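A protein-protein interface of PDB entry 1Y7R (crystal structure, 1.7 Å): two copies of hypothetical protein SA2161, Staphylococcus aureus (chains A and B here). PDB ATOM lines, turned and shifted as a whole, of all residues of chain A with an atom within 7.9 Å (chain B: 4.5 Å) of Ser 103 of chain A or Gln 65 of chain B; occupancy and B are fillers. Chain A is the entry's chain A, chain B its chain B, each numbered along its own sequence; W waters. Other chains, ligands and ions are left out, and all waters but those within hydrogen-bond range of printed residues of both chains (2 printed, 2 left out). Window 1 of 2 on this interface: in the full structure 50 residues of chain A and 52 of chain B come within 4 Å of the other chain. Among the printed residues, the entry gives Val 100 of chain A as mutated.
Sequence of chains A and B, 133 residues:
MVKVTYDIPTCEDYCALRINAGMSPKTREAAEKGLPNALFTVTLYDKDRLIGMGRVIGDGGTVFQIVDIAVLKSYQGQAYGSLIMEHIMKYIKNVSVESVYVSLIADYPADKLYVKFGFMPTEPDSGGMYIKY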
ATOM      1  N   ARG A  55      10.946   6.872 -16.929  1.00  0.00           N
ATOM      2  CA  ARG A  55      10.802   5.869 -17.991  1.00  0.00           C
ATOM      3  C   ARG A  55       9.857   6.410 -19.061  1.00  0.00           C
ATOM      4  O   ARG A  55       9.060   7.318 -18.791  1.00  0.00           O
ATOM      5  CB  ARG A  55      10.277   4.528 -17.416  1.00  0.00           C
ATOM      6  CG  ARG A  55      11.160   3.973 -16.289  1.00  0.00           C
ATOM      7  CD  ARG A  55      10.564   2.796 -15.563  1.00  0.00           C
ATOM      8  NE  ARG A  55      10.493   1.591 -16.408  1.00  0.00           N
ATOM      9  CZ  ARG A  55       9.407   0.841 -16.613  1.00  0.00           C
ATOM     10  NH1 ARG A  55       8.239   1.117 -16.029  1.00  0.00           N
ATOM     11  NH2 ARG A  55       9.533  -0.234 -17.392  1.00  0.00           N
ATOM     12  N   VAL A  56       9.991   5.881 -20.271  1.00  0.00           N
ATOM     13  CA  VAL A  56       9.114   6.218 -21.403  1.00  0.00           C
ATOM     14  C   VAL A  56       8.586   4.919 -22.050  1.00  0.00           C
ATOM     15  O   VAL A  56       9.352   3.977 -22.342  1.00  0.00           O
ATOM     16  CB  VAL A  56       9.857   7.057 -22.451  1.00  0.00           C
ATOM     17  CG1 VAL A  56       8.960   7.344 -23.690  1.00  0.00           C
ATOM     18  CG2 VAL A  56      10.387   8.351 -21.839  1.00  0.00           C
ATOM     19  N   ILE A  57       7.270   4.890 -22.277  1.00  0.00           N
ATOM     20  CA  ILE A  57       6.608   3.879 -23.085  1.00  0.00           C
ATOM     21  C   ILE A  57       6.054   4.582 -24.337  1.00  0.00           C
ATOM     22  O   ILE A  57       5.913   5.814 -24.362  1.00  0.00           O
ATOM     23  CB  ILE A  57       5.492   3.125 -22.311  1.00  0.00           C
ATOM     24  CG1 ILE A  57       4.447   4.099 -21.720  1.00  0.00           C
ATOM     25  CG2 ILE A  57       6.111   2.227 -21.208  1.00  0.00           C
ATOM     26  CD1 ILE A  57       3.111   3.442 -21.359  1.00  0.00           C
ATOM     27  N   GLY A  58       5.729   3.816 -25.360  1.00  0.00           N
ATOM     28  CA  GLY A  58       5.206   4.473 -26.565  1.00  0.00           C
ATOM     29  C   GLY A  58       5.237   3.559 -27.772  1.00  0.00           C
ATOM     30  O   GLY A  58       5.550   2.366 -27.647  1.00  0.00           O
ATOM     31  N   VAL A  63       2.721   8.277 -30.421  1.00  0.00           N
ATOM     32  CA  VAL A  63       2.360   8.507 -29.023  1.00  0.00           C
ATOM     33  C   VAL A  63       3.446   7.987 -28.069  1.00  0.00           C
ATOM     34  O   VAL A  63       3.987   6.906 -28.284  1.00  0.00           O
ATOM     35  CB  VAL A  63       0.986   7.872 -28.694  1.00  0.00           C
ATOM     36  CG1 VAL A  63       0.966   6.334 -28.950  1.00  0.00           C
ATOM     37  CG2 VAL A  63       0.488   8.274 -27.295  1.00  0.00           C
ATOM     38  N   PHE A  64       3.728   8.774 -27.034  1.00  0.00           N
ATOM     39  CA  PHE A  64       4.551   8.321 -25.893  1.00  0.00           C
ATOM     40  C   PHE A  64       3.876   8.711 -24.570  1.00  0.00           C
ATOM     41  O   PHE A  64       3.114   9.687 -24.508  1.00  0.00           O
ATOM     42  CB  PHE A  64       5.943   8.971 -25.942  1.00  0.00           C
ATOM     43  CG  PHE A  64       6.715   8.673 -27.203  1.00  0.00           C
ATOM     44  CD1 PHE A  64       7.639   7.640 -27.217  1.00  0.00           C
ATOM     45  CD2 PHE A  64       6.512   9.444 -28.361  1.00  0.00           C
ATOM     46  CE1 PHE A  64       8.382   7.345 -28.398  1.00  0.00           C
ATOM     47  CE2 PHE A  64       7.244   9.181 -29.531  1.00  0.00           C
ATOM     48  CZ  PHE A  64       8.161   8.104 -29.559  1.00  0.00           C
ATOM     49  N   GLN A  65       4.184   7.953 -23.517  1.00  0.00           N
ATOM     50  CA  GLN A  65       3.795   8.339 -22.168  1.00  0.00           C
ATOM     51  C   GLN A  65       5.036   8.278 -21.295  1.00  0.00           C
ATOM     52  O   GLN A  65       5.769   7.285 -21.318  1.00  0.00           O
ATOM     53  CB  GLN A  65       2.737   7.396 -21.586  1.00  0.00           C
ATOM     54  CG  GLN A  65       1.999   8.041 -20.402  1.00  0.00           C
ATOM     55  CD  GLN A  65       1.091   7.090 -19.654  1.00  0.00           C
ATOM     56  OE1 GLN A  65       1.223   5.872 -19.721  1.00  0.00           O
ATOM     57  NE2 GLN A  65       0.199   7.661 -18.880  1.00  0.00           N
ATOM     58  N   ILE A  66       5.256   9.345 -20.544  1.00  0.00           N
ATOM     59  CA  ILE A  66       6.319   9.413 -19.552  1.00  0.00           C
ATOM     60  C   ILE A  66       5.728   8.891 -18.250  1.00  0.00           C
ATOM     61  O   ILE A  66       4.632   9.331 -17.837  1.00  0.00           O
ATOM     62  CB  ILE A  66       6.816  10.858 -19.382  1.00  0.00           C
ATOM     63  CG1 ILE A  66       7.383  11.344 -20.718  1.00  0.00           C
ATOM     64  CG2 ILE A  66       7.845  10.968 -18.254  1.00  0.00           C
ATOM     65  CD1 ILE A  66       7.669  12.812 -20.755  1.00  0.00           C
ATOM     66  N   VAL A  67       6.444   7.951 -17.631  1.00  0.00           N
ATOM     67  CA  VAL A  67       5.942   7.234 -16.454  1.00  0.00           C
ATOM     68  C   VAL A  67       7.063   7.064 -15.437  1.00  0.00           C
ATOM     69  O   VAL A  67       8.224   7.205 -15.799  1.00  0.00           O
ATOM     70  CB  VAL A  67       5.342   5.831 -16.819  1.00  0.00           C
ATOM     71  CG1 VAL A  67       4.125   5.963 -17.756  1.00  0.00           C
ATOM     72  CG2 VAL A  67       6.421   4.839 -17.407  1.00  0.00           C
ATOM     73  N   ILE A  92      13.078  11.767 -26.445  1.00  0.00           N
ATOM     74  CA  ILE A  92      11.861  11.972 -27.250  1.00  0.00           C
ATOM     75  C   ILE A  92      12.148  12.881 -28.461  1.00  0.00           C
ATOM     76  O   ILE A  92      11.679  12.596 -29.564  1.00  0.00           O
ATOM     77  CB  ILE A  92      10.706  12.509 -26.396  1.00  0.00           C
ATOM     78  CG1 ILE A  92      10.321  11.459 -25.332  1.00  0.00           C
ATOM     79  CG2 ILE A  92       9.496  12.836 -27.296  1.00  0.00           C
ATOM     80  CD1 ILE A  92       9.302  11.961 -24.274  1.00  0.00           C
ATOM     81  N   VAL A 100       3.575  14.056 -33.239  1.00  0.00           N
ATOM     82  CA  VAL A 100       3.785  13.140 -32.104  1.00  0.00           C
ATOM     83  C   VAL A 100       3.180  13.761 -30.850  1.00  0.00           C
ATOM     84  O   VAL A 100       3.388  14.931 -30.590  1.00  0.00           O
ATOM     85  CB  VAL A 100       5.291  12.877 -31.883  1.00  0.00           C
ATOM     86  CG1 VAL A 100       5.545  12.056 -30.606  1.00  0.00           C
ATOM     87  CG2 VAL A 100       5.860  12.165 -33.061  1.00  0.00           C
ATOM     88  N   TYR A 101       2.497  12.930 -30.070  1.00  0.00           N
ATOM     89  CA  TYR A 101       1.837  13.327 -28.828  1.00  0.00           C
ATOM     90  C   TYR A 101       2.564  12.695 -27.656  1.00  0.00           C
ATOM     91  O   TYR A 101       2.867  11.485 -27.689  1.00  0.00           O
ATOM     92  CB  TYR A 101       0.437  12.771 -28.850  1.00  0.00           C
ATOM     93  CG  TYR A 101      -0.430  13.081 -27.658  1.00  0.00           C
ATOM     94  CD1 TYR A 101      -1.153  14.280 -27.587  1.00  0.00           C
ATOM     95  CD2 TYR A 101      -0.585  12.140 -26.634  1.00  0.00           C
ATOM     96  CE1 TYR A 101      -1.991  14.544 -26.500  1.00  0.00           C
ATOM     97  CE2 TYR A 101      -1.409  12.394 -25.535  1.00  0.00           C
ATOM     98  CZ  TYR A 101      -2.109  13.611 -25.486  1.00  0.00           C
ATOM     99  OH  TYR A 101      -2.940  13.868 -24.422  1.00  0.00           O
ATOM    100  N   VAL A 102       2.841  13.477 -26.612  1.00  0.00           N
ATOM    101  CA  VAL A 102       3.432  12.861 -25.416  1.00  0.00           C
ATOM    102  C   VAL A 102       2.587  13.278 -24.230  1.00  0.00           C
ATOM    103  O   VAL A 102       2.196  14.449 -24.116  1.00  0.00           O
ATOM    104  CB  VAL A 102       4.873  13.349 -25.185  1.00  0.00           C
ATOM    105  CG1 VAL A 102       5.500  12.641 -23.955  1.00  0.00           C
ATOM    106  CG2 VAL A 102       5.759  13.174 -26.456  1.00  0.00           C
ATOM    107  N   SER A 103       2.255  12.335 -23.361  1.00  0.00           N
ATOM    108  CA  SER A 103       1.451  12.699 -22.202  1.00  0.00           C
ATOM    109  C   SER A 103       2.003  12.113 -20.920  1.00  0.00           C
ATOM    110  O   SER A 103       2.839  11.189 -20.943  1.00  0.00           O
ATOM    111  CB  SER A 103      -0.030  12.290 -22.391  1.00  0.00           C
ATOM    112  OG  SER A 103      -0.259  10.904 -22.108  1.00  0.00           O
ATOM    113  N   LEU A 104       1.480  12.618 -19.810  1.00  0.00           N
ATOM    114  CA  LEU A 104       1.786  12.048 -18.505  1.00  0.00           C
ATOM    115  C   LEU A 104       0.657  12.342 -17.535  1.00  0.00           C
ATOM    116  O   LEU A 104      -0.243  13.123 -17.859  1.00  0.00           O
ATOM    117  CB  LEU A 104       3.113  12.597 -17.978  1.00  0.00           C
ATOM    118  CG  LEU A 104       3.280  14.114 -17.931  1.00  0.00           C
ATOM    119  CD1 LEU A 104       2.715  14.655 -16.635  1.00  0.00           C
ATOM    120  CD2 LEU A 104       4.750  14.443 -18.044  1.00  0.00           C
ATOM    121  N   ILE A 105       0.711  11.695 -16.364  1.00  0.00           N
ATOM    122  CA  ILE A 105      -0.278  11.932 -15.297  1.00  0.00           C
ATOM    123  C   ILE A 105       0.457  12.562 -14.127  1.00  0.00           C
ATOM    124  O   ILE A 105       1.446  12.016 -13.634  1.00  0.00           O
ATOM    125  CB  ILE A 105      -0.963  10.612 -14.859  1.00  0.00           C
ATOM    126  CG1 ILE A 105      -1.698   9.932 -16.030  1.00  0.00           C
ATOM    127  CG2 ILE A 105      -1.848  10.819 -13.640  1.00  0.00           C
ATOM    128  CD1 ILE A 105      -2.732  10.784 -16.690  1.00  0.00           C
ATOM    129  N   ALA A 106       0.011  13.738 -13.706  1.00  0.00           N
ATOM    130  CA  ALA A 106       0.714  14.467 -12.663  1.00  0.00           C
ATOM    131  C   ALA A 106      -0.208  14.857 -11.530  1.00  0.00           C
ATOM    132  O   ALA A 106      -1.272  15.385 -11.788  1.00  0.00           O
ATOM    133  CB  ALA A 106       1.325  15.724 -13.274  1.00  0.00           C
ATOM    134  N   PHE A 119       4.886  21.040 -20.886  1.00  0.00           N
ATOM    135  CA  PHE A 119       3.617  20.296 -20.706  1.00  0.00           C
ATOM    136  C   PHE A 119       2.490  21.219 -20.254  1.00  0.00           C
ATOM    137  O   PHE A 119       2.712  22.159 -19.492  1.00  0.00           O
ATOM    138  CB  PHE A 119       3.809  19.140 -19.717  1.00  0.00           C
ATOM    139  CG  PHE A 119       4.562  18.012 -20.314  1.00  0.00           C
ATOM    140  CD1 PHE A 119       3.882  16.983 -20.962  1.00  0.00           C
ATOM    141  CD2 PHE A 119       5.959  18.002 -20.319  1.00  0.00           C
ATOM    142  CE1 PHE A 119       4.591  15.928 -21.571  1.00  0.00           C
ATOM    143  CE2 PHE A 119       6.655  16.962 -20.952  1.00  0.00           C
ATOM    144  CZ  PHE A 119       5.965  15.935 -21.586  1.00  0.00           C
ATOM    145  N   MET A 120       1.292  20.958 -20.760  1.00  0.00           N
ATOM    146  CA  MET A 120       0.123  21.711 -20.341  1.00  0.00           C
ATOM    147  C   MET A 120      -1.014  20.748 -19.995  1.00  0.00           C
ATOM    148  O   MET A 120      -1.013  19.588 -20.427  1.00  0.00           O
ATOM    149  CB  MET A 120      -0.299  22.642 -21.454  1.00  0.00           C
ATOM    150  CG  MET A 120      -0.440  21.904 -22.740  1.00  0.00           C
ATOM    151  SD  MET A 120      -1.472  22.865 -23.928  1.00  0.00           S
ATOM    152  CE  MET A 120      -0.088  24.131 -24.637  1.00  0.00           C
ATOM    153  N   THR A 122      -4.326  18.589 -19.903  1.00  0.00           N
ATOM    154  CA  THR A 122      -5.326  18.086 -20.833  1.00  0.00           C
ATOM    155  C   THR A 122      -6.714  18.662 -20.506  1.00  0.00           C
ATOM    156  O   THR A 122      -7.546  18.870 -21.403  1.00  0.00           O
ATOM    157  CB  THR A 122      -5.388  16.557 -20.854  1.00  0.00           C
ATOM    158  OG1 THR A 122      -5.707  16.062 -19.538  1.00  0.00           O
ATOM    159  CG2 THR A 122      -4.043  15.992 -21.322  1.00  0.00           C
ATOM    160  N   GLY A 128      -7.330  12.227 -17.812  1.00  0.00           N
ATOM    161  CA  GLY A 128      -6.857  10.894 -17.483  1.00  0.00           C
ATOM    162  C   GLY A 128      -7.962  10.059 -16.848  1.00  0.00           C
ATOM    163  O   GLY A 128      -8.784  10.561 -16.061  1.00  0.00           O
ATOM    164  N   MET A 129      -7.996   8.781 -17.232  1.00  0.00           N
ATOM    165  CA  MET A 129      -8.805   7.776 -16.537  1.00  0.00           C
ATOM    166  C   MET A 129      -7.944   6.548 -16.323  1.00  0.00           C
ATOM    167  O   MET A 129      -7.013   6.297 -17.105  1.00  0.00           O
ATOM    168  CB  MET A 129     -10.062   7.411 -17.325  1.00  0.00           C
ATOM    169  CG  MET A 129     -10.858   8.639 -17.725  1.00  0.00           C
ATOM    170  SD  MET A 129     -12.529   8.133 -18.570  1.00  0.00           S
ATOM    171  CE  MET A 129     -13.402   7.476 -17.029  1.00  0.00           C
ATOM    172  N   ARG B  55      -5.646   0.656 -29.772  1.00  0.00           N
ATOM    173  CA  ARG B  55      -4.259   0.205 -29.603  1.00  0.00           C
ATOM    174  C   ARG B  55      -3.841   0.284 -28.137  1.00  0.00           C
ATOM    175  O   ARG B  55      -4.449   1.014 -27.334  1.00  0.00           O
ATOM    176  CB  ARG B  55      -3.301   1.037 -30.477  1.00  0.00           C
ATOM    177  CG  ARG B  55      -3.693   1.019 -31.970  1.00  0.00           C
ATOM    178  CD  ARG B  55      -2.950   2.069 -32.808  1.00  0.00           C
ATOM    179  NE  ARG B  55      -1.524   1.770 -32.973  1.00  0.00           N
ATOM    180  CZ  ARG B  55      -0.512   2.590 -32.693  1.00  0.00           C
ATOM    181  NH1 ARG B  55      -0.701   3.821 -32.191  1.00  0.00           N
ATOM    182  NH2 ARG B  55       0.728   2.178 -32.925  1.00  0.00           N
ATOM    183  N   VAL B  56      -2.781  -0.453 -27.821  1.00  0.00           N
ATOM    184  CA  VAL B  56      -2.150  -0.453 -26.505  1.00  0.00           C
ATOM    185  C   VAL B  56      -0.646  -0.271 -26.588  1.00  0.00           C
ATOM    186  O   VAL B  56       0.025  -0.924 -27.406  1.00  0.00           O
ATOM    187  CB  VAL B  56      -2.433  -1.796 -25.773  1.00  0.00           C
ATOM    188  CG1 VAL B  56      -1.862  -1.788 -24.392  1.00  0.00           C
ATOM    189  CG2 VAL B  56      -3.941  -2.109 -25.757  1.00  0.00           C
ATOM    190  N   ILE B  57      -0.120   0.633 -25.759  1.00  0.00           N
ATOM    191  CA  ILE B  57       1.320   0.721 -25.520  1.00  0.00           C
ATOM    192  C   ILE B  57       1.574   0.370 -24.063  1.00  0.00           C
ATOM    193  O   ILE B  57       0.639   0.317 -23.275  1.00  0.00           O
ATOM    194  CB  ILE B  57       1.872   2.100 -25.874  1.00  0.00           C
ATOM    195  CG1 ILE B  57       1.136   3.206 -25.081  1.00  0.00           C
ATOM    196  CG2 ILE B  57       1.704   2.337 -27.387  1.00  0.00           C
ATOM    197  CD1 ILE B  57       1.761   4.581 -25.129  1.00  0.00           C
ATOM    198  N   PHE B  64       0.352   0.234 -18.683  1.00  0.00           N
ATOM    199  CA  PHE B  64      -0.171   0.275 -20.062  1.00  0.00           C
ATOM    200  C   PHE B  64      -0.915   1.571 -20.263  1.00  0.00           C
ATOM    201  O   PHE B  64      -1.471   2.115 -19.300  1.00  0.00           O
ATOM    202  CB  PHE B  64      -1.105  -0.910 -20.318  1.00  0.00           C
ATOM    203  CG  PHE B  64      -0.445  -2.239 -20.129  1.00  0.00           C
ATOM    204  CD1 PHE B  64       0.100  -2.917 -21.228  1.00  0.00           C
ATOM    205  CD2 PHE B  64      -0.348  -2.809 -18.857  1.00  0.00           C
ATOM    206  CE1 PHE B  64       0.705  -4.159 -21.052  1.00  0.00           C
ATOM    207  CE2 PHE B  64       0.256  -4.045 -18.661  1.00  0.00           C
ATOM    208  CZ  PHE B  64       0.807  -4.719 -19.753  1.00  0.00           C
ATOM    209  N   GLN B  65      -0.949   2.054 -21.511  1.00  0.00           N
ATOM    210  CA  GLN B  65      -1.866   3.115 -21.900  1.00  0.00           C
ATOM    211  C   GLN B  65      -2.662   2.649 -23.096  1.00  0.00           C
ATOM    212  O   GLN B  65      -2.113   2.140 -24.085  1.00  0.00           O
ATOM    213  CB  GLN B  65      -1.131   4.431 -22.240  1.00  0.00           C
ATOM    214  CG  GLN B  65      -2.056   5.666 -22.290  1.00  0.00           C
ATOM    215  CD  GLN B  65      -1.290   6.949 -22.633  1.00  0.00           C
ATOM    216  OE1 GLN B  65      -0.376   6.937 -23.463  1.00  0.00           O
ATOM    217  NE2 GLN B  65      -1.680   8.059 -22.031  1.00  0.00           N
ATOM    218  N   ILE B  66      -3.966   2.841 -23.016  1.00  0.00           N
ATOM    219  CA  ILE B  66      -4.831   2.558 -24.165  1.00  0.00           C
ATOM    220  C   ILE B  66      -4.888   3.813 -25.019  1.00  0.00           C
ATOM    221  O   ILE B  66      -5.132   4.910 -24.510  1.00  0.00           O
ATOM    222  CB  ILE B  66      -6.221   2.150 -23.689  1.00  0.00           C
ATOM    223  CG1 ILE B  66      -6.115   0.848 -22.870  1.00  0.00           C
ATOM    224  CG2 ILE B  66      -7.168   2.022 -24.871  1.00  0.00           C
ATOM    225  CD1 ILE B  66      -7.381   0.420 -22.240  1.00  0.00           C
ATOM    226  N   VAL B  67      -4.686   3.652 -26.328  1.00  0.00           N
ATOM    227  CA  VAL B  67      -4.617   4.789 -27.237  1.00  0.00           C
ATOM    228  C   VAL B  67      -5.392   4.545 -28.530  1.00  0.00           C
ATOM    229  O   VAL B  67      -5.673   3.398 -28.889  1.00  0.00           O
ATOM    230  CB  VAL B  67      -3.140   5.135 -27.564  1.00  0.00           C
ATOM    231  CG1 VAL B  67      -2.359   5.546 -26.284  1.00  0.00           C
ATOM    232  CG2 VAL B  67      -2.417   3.971 -28.252  1.00  0.00           C
ATOM    233  N   SER B 103      -3.961   3.296 -17.991  1.00  0.00           N
ATOM    234  CA  SER B 103      -4.634   4.576 -18.062  1.00  0.00           C
ATOM    235  C   SER B 103      -4.906   4.936 -19.501  1.00  0.00           C
ATOM    236  O   SER B 103      -4.461   4.247 -20.425  1.00  0.00           O
ATOM    237  CB  SER B 103      -3.845   5.677 -17.339  1.00  0.00           C
ATOM    238  OG  SER B 103      -2.731   6.101 -18.120  1.00  0.00           O
ATOM    239  N   LEU B 104      -5.616   6.036 -19.689  1.00  0.00           N
ATOM    240  CA  LEU B 104      -5.858   6.561 -21.024  1.00  0.00           C
ATOM    241  C   LEU B 104      -6.157   8.039 -20.890  1.00  0.00           C
ATOM    242  O   LEU B 104      -6.356   8.522 -19.796  1.00  0.00           O
ATOM    243  CB  LEU B 104      -7.027   5.841 -21.697  1.00  0.00           C
ATOM    244  CG  LEU B 104      -8.310   5.722 -20.902  1.00  0.00           C
ATOM    245  CD1 LEU B 104      -9.212   6.982 -21.068  1.00  0.00           C
ATOM    246  CD2 LEU B 104      -9.000   4.438 -21.376  1.00  0.00           C
ATOM    247  N   ILE B 105      -6.115   8.758 -22.009  1.00  0.00           N
ATOM    248  CA  ILE B 105      -6.579  10.134 -22.052  1.00  0.00           C
ATOM    249  C   ILE B 105      -7.880  10.122 -22.846  1.00  0.00           C
ATOM    250  O   ILE B 105      -7.898   9.686 -24.027  1.00  0.00           O
ATOM    251  CB  ILE B 105      -5.575  11.095 -22.736  1.00  0.00           C
ATOM    252  CG1 ILE B 105      -4.233  11.133 -21.999  1.00  0.00           C
ATOM    253  CG2 ILE B 105      -6.212  12.524 -22.860  1.00  0.00           C
ATOM    254  CD1 ILE B 105      -4.281  11.693 -20.556  1.00  0.00           C
ATOM    255  N   MET B 129      -1.324  15.732 -18.473  1.00  0.00           N
ATOM    256  CA  MET B 129      -0.650  16.836 -19.144  1.00  0.00           C
ATOM    257  C   MET B 129      -0.039  16.342 -20.430  1.00  0.00           C
ATOM    258  O   MET B 129       0.263  15.148 -20.582  1.00  0.00           O
ATOM    259  CB  MET B 129       0.444  17.435 -18.261  1.00  0.00           C
ATOM    260  CG  MET B 129      -0.037  17.767 -16.871  1.00  0.00           C
ATOM    261  SD  MET B 129       1.371  18.650 -15.857  1.00  0.00           S
ATOM    262  CE  MET B 129       1.326  20.410 -16.710  1.00  0.00           C
ATOM    263  N   TYR B 130       0.151  17.250 -21.370  1.00  0.00           N
ATOM    264  CA  TYR B 130       0.630  16.795 -22.674  1.00  0.00           C
ATOM    265  C   TYR B 130       1.450  17.837 -23.397  1.00  0.00           C
ATOM    266  O   TYR B 130       1.446  19.017 -23.042  1.00  0.00           O
ATOM    267  CB  TYR B 130      -0.574  16.369 -23.562  1.00  0.00           C
ATOM    268  CG  TYR B 130      -1.303  17.527 -24.191  1.00  0.00           C
ATOM    269  CD1 TYR B 130      -1.135  17.819 -25.546  1.00  0.00           C
ATOM    270  CD2 TYR B 130      -2.124  18.377 -23.422  1.00  0.00           C
ATOM    271  CE1 TYR B 130      -1.796  18.905 -26.137  1.00  0.00           C
ATOM    272  CE2 TYR B 130      -2.796  19.459 -24.020  1.00  0.00           C
ATOM    273  CZ  TYR B 130      -2.603  19.712 -25.368  1.00  0.00           C
ATOM    274  OH  TYR B 130      -3.259  20.783 -25.971  1.00  0.00           O
HETATM  275  O   HOH W   1       0.261   9.370 -24.240  1.00  0.00           O
HETATM  276  O   HOH W   2      -0.615   4.521 -18.203  1.00  0.00           O
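The side-chain amide nitrogen of Gln 65 of chain A sits at hydrogen-bond distance from the side-chain hydroxyl of Ser 103 of chain B (3.4 Å). The side-chain hydroxyl of Ser 103 of chain A sits at hydrogen-bond distance from the side-chain amide nitrogen of Gln 65 of chain B. The backbone NH of Met 129 of chain B sits at hydrogen-bond distance from the backbone carbonyl oxygen of Leu 104 of chain A (2.9 Å). The backbone carbonyl oxygen (O) of Met 120 of chain A lies within hydrogen-bond range of the backbone NH (N) of Tyr 130 of chain B (2.8 Å). The backbone NH of Leu 104 of chain B is in hydrogen-bond range of the backbone carbonyl oxygen of Met 129 of chain A (2.9 Å).
Water W1 lies within hydrogen-bond range of the side-chain amide oxygen of Gln 65 of chain B (2.6 Å), the side-chain hydroxyl of Ser 103 of chain A (2.7 Å) and the backbone carbonyl oxygen of Phe 64 of chain A (2.9 Å). Water W2 lies within hydrogen-bond range of OG of Ser 103 of chain B (2.6 Å), OE1 of Gln 65 of chain A (2.7 Å) and O of Phe 64 of chain B (2.8 Å).
Printed residues of chain A that touch a printed residue of chain B: Gly 58, Gln 65, Tyr 101, Val 102, Ser 103, Leu 104, Ala 106, Phe 119, Met 120, Thr 122, Gly 128 and Met 129. Of the 12 printed residues of chain B, 7 touch a printed residue of chain A.
Tyr 101 of chain A touches Ile 105 of chain B. Tyr 101 of chain A touches Tyr 130 of chain B. Val 102 of chain A touches Tyr 130 of chain B. Ile 105 of chain B touches Ser 103 of chain A. CB of Ala 106 of chain A touches SD of Met 129 of chain B, 3.9 Å away. Phe 119 of chain A touches Met 129 of chain B (O to CE, 3.6 Å). Tyr 130 of chain B touches Phe 119 of chain A (O to CA, 3.4 Å). Met 120 of chain A touches Met 129 of chain B. O of Leu 104 of chain B touches CA of Gly 128 of chain A, 3.4 Å away. Met 129 of chain A touches Ser 103 of chain B (O to CA, 3.1 Å).
Gln 65 of chain A touches its own counterpart, Gln 65 of chain B. Gln 65 of chain A touches Ser 103 of chain B, and with the chains exchanged Ser 103 of chain A touches Gln 65 of chain B. Ser 103 of chain A touches Met 129 of chain B, and with the chains exchanged Met 129 of chain A touches Ser 103 of chain B. Leu 104 of chain A touches Met 129 of chain B, and with the chains exchanged Met 129 of chain A touches Leu 104 of chain B. Of the 20 pairs that touch across the chains among the printed residues, 7 have their exchanged pair printed and touching as well.
Of the printed residues of chain B, Ser 103 of chain A touches Gln 65 (3.2 Å), Ile 105 (3.98 Å) and Met 129 (3.2 Å). Of the printed residues of chain B, Phe 119 of chain A touches Met 129 (3.6 Å) and Tyr 130 (3.4 Å). Val 56 of chain B touches none of the printed residues of chain A. Gln 65 of chain B touches two residues of chain A. Of the printed residues of chain A, Leu 104 of chain B touches Gly 128 and Met 129. The nearest printed residue of chain B that does not touch Ser 103 of chain A is Tyr 130 of chain B (4.2 Å).
The backbone NH of Gln 65 of chain A is in hydrogen-bond range of the backbone carbonyl oxygen of Ile 57 of chain A, 2.9 Å away. The backbone NH (N) of Phe 64 of chain A sits at hydrogen-bond distance from the backbone carbonyl oxygen (O) of Tyr 101 of chain A (2.9 Å). The backbone NH (N) of Ser 103 of chain A is in hydrogen-bond range of the backbone carbonyl oxygen (O) of Phe 64 of chain A (3.0 Å). N of Gln 65 of chain B is in hydrogen-bond range of O of Ile 57 of chain B (2.9 Å). O of Phe 64 of chain B is in hydrogen-bond range of N of Ser 103 of chain B (3.1 Å). The backbone carbonyl oxygen (O) of Ser 103 of chain B is in hydrogen-bond range of the backbone NH (N) of Ile 66 of chain B.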
